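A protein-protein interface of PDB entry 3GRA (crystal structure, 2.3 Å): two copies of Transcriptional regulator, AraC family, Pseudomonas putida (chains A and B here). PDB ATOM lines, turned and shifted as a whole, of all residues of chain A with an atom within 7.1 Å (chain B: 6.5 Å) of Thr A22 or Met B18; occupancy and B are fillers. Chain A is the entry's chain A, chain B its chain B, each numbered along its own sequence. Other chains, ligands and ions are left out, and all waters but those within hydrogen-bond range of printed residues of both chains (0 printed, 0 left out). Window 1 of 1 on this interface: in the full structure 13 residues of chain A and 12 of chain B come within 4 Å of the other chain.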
ATOM      1  N   PHE A  16      15.904  -7.072   0.128  1.00  0.00           N
ATOM      2  CA  PHE A  16      14.503  -7.065  -0.281  1.00  0.00           C
ATOM      3  C   PHE A  16      14.206  -8.251  -1.201  1.00  0.00           C
ATOM      4  O   PHE A  16      15.047  -8.652  -2.014  1.00  0.00           O
ATOM      5  CB  PHE A  16      14.190  -5.760  -1.020  1.00  0.00           C
ATOM      6  CG  PHE A  16      14.835  -5.658  -2.390  1.00  0.00           C
ATOM      7  CD1 PHE A  16      14.162  -6.104  -3.526  1.00  0.00           C
ATOM      8  CD2 PHE A  16      16.100  -5.090  -2.541  1.00  0.00           C
ATOM      9  CE1 PHE A  16      14.732  -5.980  -4.793  1.00  0.00           C
ATOM     10  CE2 PHE A  16      16.684  -4.959  -3.802  1.00  0.00           C
ATOM     11  CZ  PHE A  16      16.000  -5.404  -4.937  1.00  0.00           C
ATOM     12  N   SER A  17      13.016  -8.819  -1.057  1.00  0.00           N
ATOM     13  CA  SER A  17      12.604  -9.928  -1.908  1.00  0.00           C
ATOM     14  C   SER A  17      12.622  -9.436  -3.364  1.00  0.00           C
ATOM     15  O   SER A  17      11.825  -8.581  -3.751  1.00  0.00           O
ATOM     16  CB  SER A  17      11.201 -10.367  -1.514  1.00  0.00           C
ATOM     17  OG  SER A  17      10.677 -11.243  -2.487  1.00  0.00           O
ATOM     18  N   MET A  18      13.535  -9.951  -4.175  1.00  0.00           N
ATOM     19  CA  MET A  18      13.610  -9.485  -5.562  1.00  0.00           C
ATOM     20  C   MET A  18      12.413  -9.915  -6.402  1.00  0.00           C
ATOM     21  O   MET A  18      11.956  -9.174  -7.280  1.00  0.00           O
ATOM     22  CB  MET A  18      14.896  -9.984  -6.241  1.00  0.00           C
ATOM     23  CG  MET A  18      14.983  -9.608  -7.715  1.00  0.00           C
ATOM     24  SD  MET A  18      15.378  -7.879  -8.011  1.00  0.00           S
ATOM     25  CE  MET A  18      17.147  -8.079  -8.191  1.00  0.00           C
ATOM     26  N   ALA A  19      11.927 -11.119  -6.125  1.00  0.00           N
ATOM     27  CA  ALA A  19      10.791 -11.695  -6.829  1.00  0.00           C
ATOM     28  C   ALA A  19       9.507 -10.917  -6.519  1.00  0.00           C
ATOM     29  O   ALA A  19       8.629 -10.791  -7.375  1.00  0.00           O
ATOM     30  CB  ALA A  19      10.626 -13.163  -6.432  1.00  0.00           C
ATOM     31  N   SER A  20       9.398 -10.414  -5.292  1.00  0.00           N
ATOM     32  CA  SER A  20       8.225  -9.647  -4.920  1.00  0.00           C
ATOM     33  C   SER A  20       8.252  -8.345  -5.709  1.00  0.00           C
ATOM     34  O   SER A  20       7.266  -7.942  -6.332  1.00  0.00           O
ATOM     35  CB  SER A  20       8.227  -9.338  -3.415  1.00  0.00           C
ATOM     36  OG  SER A  20       7.937 -10.493  -2.665  1.00  0.00           O
ATOM     37  N   PHE A  21       9.407  -7.700  -5.694  1.00  0.00           N
ATOM     38  CA  PHE A  21       9.558  -6.434  -6.387  1.00  0.00           C
ATOM     39  C   PHE A  21       9.410  -6.516  -7.910  1.00  0.00           C
ATOM     40  O   PHE A  21       8.698  -5.714  -8.507  1.00  0.00           O
ATOM     41  CB  PHE A  21      10.903  -5.804  -6.044  1.00  0.00           C
ATOM     42  CG  PHE A  21      11.143  -4.496  -6.734  1.00  0.00           C
ATOM     43  CD1 PHE A  21      10.271  -3.426  -6.546  1.00  0.00           C
ATOM     44  CD2 PHE A  21      12.227  -4.336  -7.582  1.00  0.00           C
ATOM     45  CE1 PHE A  21      10.482  -2.225  -7.195  1.00  0.00           C
ATOM     46  CE2 PHE A  21      12.446  -3.131  -8.239  1.00  0.00           C
ATOM     47  CZ  PHE A  21      11.578  -2.077  -8.049  1.00  0.00           C
ATOM     48  N   THR A  22      10.082  -7.479  -8.534  1.00  0.00           N
ATOM     49  CA  THR A  22      10.024  -7.613  -9.984  1.00  0.00           C
ATOM     50  C   THR A  22       8.650  -8.035 -10.510  1.00  0.00           C
ATOM     51  O   THR A  22       8.240  -7.594 -11.584  1.00  0.00           O
ATOM     52  CB  THR A  22      11.090  -8.601 -10.502  1.00  0.00           C
ATOM     53  OG1 THR A  22      10.826  -9.913  -9.991  1.00  0.00           O
ATOM     54  CG2 THR A  22      12.475  -8.157 -10.063  1.00  0.00           C
ATOM     55  N   VAL A  23       7.933  -8.878  -9.778  1.00  0.00           N
ATOM     56  CA  VAL A  23       6.620  -9.261 -10.262  1.00  0.00           C
ATOM     57  C   VAL A  23       5.647  -8.074 -10.143  1.00  0.00           C
ATOM     58  O   VAL A  23       4.840  -7.832 -11.038  1.00  0.00           O
ATOM     59  CB  VAL A  23       6.061 -10.487  -9.501  1.00  0.00           C
ATOM     60  CG1 VAL A  23       5.738 -10.120  -8.066  1.00  0.00           C
ATOM     61  CG2 VAL A  23       4.822 -11.004 -10.218  1.00  0.00           C
ATOM     62  N   ALA A  24       5.725  -7.324  -9.046  1.00  0.00           N
ATOM     63  CA  ALA A  24       4.844  -6.176  -8.903  1.00  0.00           C
ATOM     64  C   ALA A  24       5.099  -5.195 -10.054  1.00  0.00           C
ATOM     65  O   ALA A  24       4.156  -4.691 -10.657  1.00  0.00           O
ATOM     66  CB  ALA A  24       5.071  -5.488  -7.572  1.00  0.00           C
ATOM     67  N   MET A  25       6.377  -4.945 -10.350  1.00  0.00           N
ATOM     68  CA  MET A  25       6.771  -4.033 -11.426  1.00  0.00           C
ATOM     69  C   MET A  25       6.300  -4.536 -12.784  1.00  0.00           C
ATOM     70  O   MET A  25       5.895  -3.756 -13.641  1.00  0.00           O
ATOM     71  CB  MET A  25       8.298  -3.855 -11.468  1.00  0.00           C
ATOM     72  CG  MET A  25       8.873  -2.863 -10.465  1.00  0.00           C
ATOM     73  SD  MET A  25       8.533  -1.135 -10.854  1.00  0.00           S
ATOM     74  CE  MET A  25       9.688  -0.840 -12.177  1.00  0.00           C
ATOM     75  N   ASP A  26       6.375  -5.842 -12.979  1.00  0.00           N
ATOM     76  CA  ASP A  26       5.945  -6.434 -14.227  1.00  0.00           C
ATOM     77  C   ASP A  26       4.490  -5.999 -14.474  1.00  0.00           C
ATOM     78  O   ASP A  26       4.158  -5.484 -15.544  1.00  0.00           O
ATOM     79  CB  ASP A  26       6.041  -7.953 -14.133  1.00  0.00           C
ATOM     80  CG  ASP A  26       6.553  -8.584 -15.410  1.00  0.00           C
ATOM     81  OD1 ASP A  26       6.723  -7.850 -16.412  1.00  0.00           O
ATOM     82  OD2 ASP A  26       6.783  -9.813 -15.413  1.00  0.00           O
ATOM     83  N   VAL A  27       3.643  -6.188 -13.465  1.00  0.00           N
ATOM     84  CA  VAL A  27       2.241  -5.812 -13.551  1.00  0.00           C
ATOM     85  C   VAL A  27       2.046  -4.358 -13.976  1.00  0.00           C
ATOM     86  O   VAL A  27       1.235  -4.069 -14.849  1.00  0.00           O
ATOM     87  CB  VAL A  27       1.519  -6.013 -12.193  1.00  0.00           C
ATOM     88  CG1 VAL A  27       0.079  -5.539 -12.293  1.00  0.00           C
ATOM     89  CG2 VAL A  27       1.579  -7.480 -11.780  1.00  0.00           C
ATOM     90  N   LEU A  28       2.786  -3.445 -13.351  1.00  0.00           N
ATOM     91  CA  LEU A  28       2.665  -2.030 -13.671  1.00  0.00           C
ATOM     92  C   LEU A  28       3.251  -1.682 -15.046  1.00  0.00           C
ATOM     93  O   LEU A  28       2.764  -0.779 -15.722  1.00  0.00           O
ATOM     94  CB  LEU A  28       3.336  -1.190 -12.577  1.00  0.00           C
ATOM     95  CG  LEU A  28       2.863  -1.470 -11.143  1.00  0.00           C
ATOM     96  CD1 LEU A  28       3.638  -0.589 -10.183  1.00  0.00           C
ATOM     97  CD2 LEU A  28       1.361  -1.226 -11.010  1.00  0.00           C
ATOM     98  N   LEU A  55      18.901 -11.889  -3.699  1.00  0.00           N
ATOM     99  CA  LEU A  55      19.523 -12.721  -4.709  1.00  0.00           C
ATOM    100  C   LEU A  55      21.008 -12.373  -4.889  1.00  0.00           C
ATOM    101  O   LEU A  55      21.663 -12.906  -5.768  1.00  0.00           O
ATOM    102  CB  LEU A  55      18.795 -12.543  -6.046  1.00  0.00           C
ATOM    103  CG  LEU A  55      17.348 -13.024  -6.227  1.00  0.00           C
ATOM    104  CD1 LEU A  55      16.909 -12.762  -7.680  1.00  0.00           C
ATOM    105  CD2 LEU A  55      17.240 -14.507  -5.916  1.00  0.00           C
ATOM    106  N   LEU A  57      22.130  -9.677  -5.998  1.00  0.00           N
ATOM    107  CA  LEU A  57      22.218  -8.640  -7.013  1.00  0.00           C
ATOM    108  C   LEU A  57      21.863  -7.263  -6.463  1.00  0.00           C
ATOM    109  O   LEU A  57      21.024  -7.132  -5.575  1.00  0.00           O
ATOM    110  CB  LEU A  57      21.271  -8.951  -8.172  1.00  0.00           C
ATOM    111  CG  LEU A  57      21.629  -9.971  -9.258  1.00  0.00           C
ATOM    112  CD1 LEU A  57      22.624 -11.015  -8.772  1.00  0.00           C
ATOM    113  CD2 LEU A  57      20.335 -10.618  -9.709  1.00  0.00           C
ATOM    114  N   LEU A  59      20.478  -3.370  -7.372  1.00  0.00           N
ATOM    115  CA  LEU A  59      19.692  -2.612  -8.347  1.00  0.00           C
ATOM    116  C   LEU A  59      20.009  -1.139  -8.184  1.00  0.00           C
ATOM    117  O   LEU A  59      20.210  -0.664  -7.063  1.00  0.00           O
ATOM    118  CB  LEU A  59      18.192  -2.777  -8.109  1.00  0.00           C
ATOM    119  CG  LEU A  59      17.474  -4.010  -8.614  1.00  0.00           C
ATOM    120  CD1 LEU A  59      17.951  -5.207  -7.842  1.00  0.00           C
ATOM    121  CD2 LEU A  59      15.982  -3.821  -8.451  1.00  0.00           C
ATOM    122  N   LEU A 107       5.658  -5.075   0.768  1.00  0.00           N
ATOM    123  CA  LEU A 107       5.806  -6.409   0.171  1.00  0.00           C
ATOM    124  C   LEU A 107       6.664  -7.269   1.092  1.00  0.00           C
ATOM    125  O   LEU A 107       7.611  -6.768   1.708  1.00  0.00           O
ATOM    126  CB  LEU A 107       6.455  -6.318  -1.225  1.00  0.00           C
ATOM    127  CG  LEU A 107       5.811  -5.331  -2.227  1.00  0.00           C
ATOM    128  CD1 LEU A 107       6.608  -5.349  -3.534  1.00  0.00           C
ATOM    129  CD2 LEU A 107       4.324  -5.697  -2.493  1.00  0.00           C
ATOM    130  N   HIS B  15      17.985  -4.374 -22.262  1.00  0.00           N
ATOM    131  CA  HIS B  15      16.569  -4.742 -22.322  1.00  0.00           C
ATOM    132  C   HIS B  15      16.325  -6.217 -22.008  1.00  0.00           C
ATOM    133  O   HIS B  15      15.278  -6.764 -22.348  1.00  0.00           O
ATOM    134  CB  HIS B  15      15.989  -4.423 -23.701  1.00  0.00           C
ATOM    135  CG  HIS B  15      16.276  -3.032 -24.175  1.00  0.00           C
ATOM    136  ND1 HIS B  15      17.556  -2.567 -24.383  1.00  0.00           N
ATOM    137  CD2 HIS B  15      15.447  -2.024 -24.536  1.00  0.00           C
ATOM    138  CE1 HIS B  15      17.505  -1.333 -24.855  1.00  0.00           C
ATOM    139  NE2 HIS B  15      16.236  -0.980 -24.959  1.00  0.00           N
ATOM    140  N   PHE B  16      17.290  -6.859 -21.359  1.00  0.00           N
ATOM    141  CA  PHE B  16      17.157  -8.272 -21.020  1.00  0.00           C
ATOM    142  C   PHE B  16      15.926  -8.514 -20.144  1.00  0.00           C
ATOM    143  O   PHE B  16      15.474  -7.623 -19.420  1.00  0.00           O
ATOM    144  CB  PHE B  16      18.412  -8.767 -20.295  1.00  0.00           C
ATOM    145  CG  PHE B  16      18.552  -8.247 -18.883  1.00  0.00           C
ATOM    146  CD1 PHE B  16      18.033  -8.964 -17.810  1.00  0.00           C
ATOM    147  CD2 PHE B  16      19.190  -7.036 -18.629  1.00  0.00           C
ATOM    148  CE1 PHE B  16      18.142  -8.487 -16.503  1.00  0.00           C
ATOM    149  CE2 PHE B  16      19.301  -6.550 -17.322  1.00  0.00           C
ATOM    150  CZ  PHE B  16      18.774  -7.283 -16.262  1.00  0.00           C
ATOM    151  N   SER B  17      15.395  -9.730 -20.230  1.00  0.00           N
ATOM    152  CA  SER B  17      14.219 -10.140 -19.473  1.00  0.00           C
ATOM    153  C   SER B  17      14.566 -10.281 -17.990  1.00  0.00           C
ATOM    154  O   SER B  17      15.247 -11.226 -17.589  1.00  0.00           O
ATOM    155  CB  SER B  17      13.711 -11.478 -20.018  1.00  0.00           C
ATOM    156  OG  SER B  17      12.447 -11.827 -19.476  1.00  0.00           O
ATOM    157  N   MET B  18      14.102  -9.341 -17.172  1.00  0.00           N
ATOM    158  CA  MET B  18      14.393  -9.404 -15.744  1.00  0.00           C
ATOM    159  C   MET B  18      13.790 -10.655 -15.121  1.00  0.00           C
ATOM    160  O   MET B  18      14.482 -11.417 -14.448  1.00  0.00           O
ATOM    161  CB  MET B  18      13.845  -8.184 -15.012  1.00  0.00           C
ATOM    162  CG  MET B  18      14.204  -8.182 -13.536  1.00  0.00           C
ATOM    163  SD  MET B  18      15.964  -7.895 -13.252  1.00  0.00           S
ATOM    164  CE  MET B  18      15.921  -6.132 -13.390  1.00  0.00           C
ATOM    165  N   ALA B  19      12.497 -10.864 -15.350  1.00  0.00           N
ATOM    166  CA  ALA B  19      11.815 -12.028 -14.802  1.00  0.00           C
ATOM    167  C   ALA B  19      12.577 -13.289 -15.181  1.00  0.00           C
ATOM    168  O   ALA B  19      12.819 -14.161 -14.348  1.00  0.00           O
ATOM    169  CB  ALA B  19      10.391 -12.095 -15.317  1.00  0.00           C
ATOM    170  N   SER B  20      12.979 -13.372 -16.443  1.00  0.00           N
ATOM    171  CA  SER B  20      13.708 -14.538 -16.917  1.00  0.00           C
ATOM    172  C   SER B  20      15.004 -14.725 -16.143  1.00  0.00           C
ATOM    173  O   SER B  20      15.295 -15.817 -15.648  1.00  0.00           O
ATOM    174  CB  SER B  20      14.005 -14.399 -18.406  1.00  0.00           C
ATOM    175  OG  SER B  20      14.738 -15.509 -18.869  1.00  0.00           O
ATOM    176  N   PHE B  21      15.785 -13.657 -16.036  1.00  0.00           N
ATOM    177  CA  PHE B  21      17.050 -13.715 -15.316  1.00  0.00           C
ATOM    178  C   PHE B  21      16.908 -13.950 -13.810  1.00  0.00           C
ATOM    179  O   PHE B  21      17.686 -14.699 -13.219  1.00  0.00           O
ATOM    180  CB  PHE B  21      17.841 -12.426 -15.541  1.00  0.00           C
ATOM    181  CG  PHE B  21      19.104 -12.343 -14.734  1.00  0.00           C
ATOM    182  CD1 PHE B  21      20.067 -13.339 -14.826  1.00  0.00           C
ATOM    183  CD2 PHE B  21      19.318 -11.284 -13.865  1.00  0.00           C
ATOM    184  CE1 PHE B  21      21.233 -13.282 -14.058  1.00  0.00           C
ATOM    185  CE2 PHE B  21      20.478 -11.211 -13.090  1.00  0.00           C
ATOM    186  CZ  PHE B  21      21.435 -12.211 -13.183  1.00  0.00           C
ATOM    187  N   THR B  22      15.927 -13.308 -13.182  1.00  0.00           N
ATOM    188  CA  THR B  22      15.744 -13.462 -11.739  1.00  0.00           C
ATOM    189  C   THR B  22      15.344 -14.869 -11.288  1.00  0.00           C
ATOM    190  O   THR B  22      15.951 -15.413 -10.357  1.00  0.00           O
ATOM    191  CB  THR B  22      14.735 -12.426 -11.192  1.00  0.00           C
ATOM    192  OG1 THR B  22      13.521 -12.483 -11.949  1.00  0.00           O
ATOM    193  CG2 THR B  22      15.320 -11.020 -11.288  1.00  0.00           C
ATOM    194  N   VAL B  23      14.350 -15.471 -11.938  1.00  0.00           N
ATOM    195  CA  VAL B  23      13.924 -16.822 -11.568  1.00  0.00           C
ATOM    196  C   VAL B  23      15.080 -17.814 -11.698  1.00  0.00           C
ATOM    197  O   VAL B  23      15.185 -18.757 -10.920  1.00  0.00           O
ATOM    198  CB  VAL B  23      12.748 -17.325 -12.443  1.00  0.00           C
ATOM    199  CG1 VAL B  23      13.183 -17.473 -13.890  1.00  0.00           C
ATOM    200  CG2 VAL B  23      12.243 -18.660 -11.906  1.00  0.00           C
ATOM    201  N   VAL B  51      23.317  -2.405 -16.534  1.00  0.00           N
ATOM    202  CA  VAL B  51      22.546  -2.848 -17.690  1.00  0.00           C
ATOM    203  C   VAL B  51      21.047  -2.600 -17.482  1.00  0.00           C
ATOM    204  O   VAL B  51      20.495  -2.904 -16.426  1.00  0.00           O
ATOM    205  CB  VAL B  51      22.780  -4.365 -17.980  1.00  0.00           C
ATOM    206  CG1 VAL B  51      22.082  -4.763 -19.268  1.00  0.00           C
ATOM    207  CG2 VAL B  51      24.269  -4.660 -18.084  1.00  0.00           C
ATOM    208  N   SER B  53      17.323  -3.411 -17.759  1.00  0.00           N
ATOM    209  CA  SER B  53      16.495  -4.603 -17.923  1.00  0.00           C
ATOM    210  C   SER B  53      15.289  -4.253 -18.777  1.00  0.00           C
ATOM    211  O   SER B  53      15.106  -3.107 -19.167  1.00  0.00           O
ATOM    212  CB  SER B  53      16.004  -5.119 -16.566  1.00  0.00           C
ATOM    213  OG  SER B  53      14.980  -4.283 -16.041  1.00  0.00           O
ATOM    214  N   ASP B  54      14.460  -5.244 -19.063  1.00  0.00           N
ATOM    215  CA  ASP B  54      13.268  -5.002 -19.857  1.00  0.00           C
ATOM    216  C   ASP B  54      12.239  -4.233 -19.031  1.00  0.00           C
ATOM    217  O   ASP B  54      11.281  -3.687 -19.574  1.00  0.00           O
ATOM    218  CB  ASP B  54      12.681  -6.337 -20.343  1.00  0.00           C
ATOM    219  CG  ASP B  54      12.018  -7.148 -19.227  1.00  0.00           C
ATOM    220  OD1 ASP B  54      12.487  -7.102 -18.065  1.00  0.00           O
ATOM    221  OD2 ASP B  54      11.029  -7.851 -19.528  1.00  0.00           O
ATOM    222  N   LEU B  55      12.450  -4.173 -17.719  1.00  0.00           N
ATOM    223  CA  LEU B  55      11.516  -3.489 -16.825  1.00  0.00           C
ATOM    224  C   LEU B  55      11.818  -2.036 -16.536  1.00  0.00           C
ATOM    225  O   LEU B  55      11.066  -1.389 -15.816  1.00  0.00           O
ATOM    226  CB  LEU B  55      11.427  -4.233 -15.493  1.00  0.00           C
ATOM    227  CG  LEU B  55      10.644  -5.543 -15.515  1.00  0.00           C
ATOM    228  CD1 LEU B  55      10.663  -6.163 -14.133  1.00  0.00           C
ATOM    229  CD2 LEU B  55       9.215  -5.273 -15.971  1.00  0.00           C
ATOM    230  N   LEU B  57      14.415  -1.151 -14.920  1.00  0.00           N
ATOM    231  CA  LEU B  57      15.341  -1.179 -13.775  1.00  0.00           C
ATOM    232  C   LEU B  57      16.744  -1.505 -14.277  1.00  0.00           C
ATOM    233  O   LEU B  57      16.909  -2.215 -15.267  1.00  0.00           O
ATOM    234  CB  LEU B  57      14.968  -2.266 -12.752  1.00  0.00           C
ATOM    235  CG  LEU B  57      13.720  -2.292 -11.849  1.00  0.00           C
ATOM    236  CD1 LEU B  57      13.394  -0.907 -11.328  1.00  0.00           C
ATOM    237  CD2 LEU B  57      12.579  -2.870 -12.619  1.00  0.00           C
ATOM    238  N   GLU B  58      17.755  -0.997 -13.586  1.00  0.00           N
ATOM    239  CA  GLU B  58      19.139  -1.263 -13.957  1.00  0.00           C
ATOM    240  C   GLU B  58      19.788  -2.090 -12.848  1.00  0.00           C
ATOM    241  O   GLU B  58      19.561  -1.827 -11.671  1.00  0.00           O
ATOM    242  CB  GLU B  58      19.915   0.049 -14.122  1.00  0.00           C
ATOM    243  CG  GLU B  58      19.585   0.865 -15.367  1.00  0.00           C
ATOM    244  CD  GLU B  58      20.226   2.256 -15.343  1.00  0.00           C
ATOM    245  OE1 GLU B  58      19.891   3.058 -14.441  1.00  0.00           O
ATOM    246  OE2 GLU B  58      21.062   2.553 -16.221  1.00  0.00           O
ATOM    247  N   LEU B  59      20.572  -3.096 -13.221  1.00  0.00           N
ATOM    248  CA  LEU B  59      21.271  -3.912 -12.239  1.00  0.00           C
ATOM    249  C   LEU B  59      22.756  -3.659 -12.404  1.00  0.00           C
ATOM    250  O   LEU B  59      23.233  -3.447 -13.517  1.00  0.00           O
ATOM    251  CB  LEU B  59      21.029  -5.411 -12.447  1.00  0.00           C
ATOM    252  CG  LEU B  59      19.639  -6.003 -12.288  1.00  0.00           C
ATOM    253  CD1 LEU B  59      18.813  -5.544 -13.468  1.00  0.00           C
ATOM    254  CD2 LEU B  59      19.707  -7.536 -12.238  1.00  0.00           C
ATOM    255  N   GLY B  79      18.978 -12.403 -22.731  1.00  0.00           N
ATOM    256  CA  GLY B  79      18.452 -11.408 -23.641  1.00  0.00           C
ATOM    257  C   GLY B  79      17.021 -11.029 -23.315  1.00  0.00           C
ATOM    258  O   GLY B  79      16.488 -11.404 -22.268  1.00  0.00           O
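N of Met B18 lies within hydrogen-bond range of OD1 of Asp B54. The backbone carbonyl oxygen of Met B18 lies within hydrogen-bond range of the side-chain hydroxyl of Thr B22 (2.9 Å). The backbone carbonyl oxygen of Ala B19 lies within hydrogen-bond range of the side-chain hydroxyl of Thr B22, 3.0 Å away. OG of Ser B53 lies close to N of Leu B55 (3.0 Å). The side-chain hydroxyl of Ser B53 lies within hydrogen-bond range of the backbone carbonyl oxygen of Leu B57 (2.9 Å). The backbone carbonyl oxygen (O) of Met A18 lies close to the side-chain hydroxyl (OG1) of Thr A22.
Among the printed residues, merely in contact across the chains: Leu A59 with Glu B58, Leu A57 with Phe B21, Met A25 with Leu B57, Asp A26 with Leu B55, Thr A22 with Leu B55, Met A18 with Thr B22, Thr A22 with Met B18, Leu A55 with Thr B22, Phe A21 with Leu B57 and Met A25 with Leu B55.
Of the 17 printed residues of chain B, 6 touch a printed residue of chain A. Printed residues of chain B that touch a printed residue of chain A: Met B18, Phe B21, Thr B22, Leu B55, Leu B57 and Glu B58. Among the printed residues, 10 pairs touch across the chains. Among the printed residues, no Asp or Glu carboxylate lies within 4 Å of a Lys or Arg side-chain nitrogen of the other chain.
Printed residues of chain B within 4 Å of Thr A22: Met B18 (3.9 Å) and Leu B55 (3.8 Å). Of chain A, only Thr A22 comes within 4 Å of Met B18. Printed residues of chain A within 4 Å of Phe B21: Leu A57 (3.4 Å). Of the printed residues of chain B, Asp A26 touches Leu B55 (3.6 Å). Of the printed residues of chain A, Glu B58 touches Leu A59 (3.4 Å). The nearest residue of chain B that does not touch Thr A22 is Thr B22 (4.2 Å).
Met A18 touches Thr B22, and with the chains exchanged Thr A22 touches Met B18. Phe A21 touches Leu B57, and with the chains exchanged Leu A57 touches Phe B21. Thr A22 touches Leu B55, and with the chains exchanged Leu A55 touches Thr B22. Positions printed for both chains: 16, 17, 18, 19, 20, 21, 22, 23, 55, 57 and 59.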
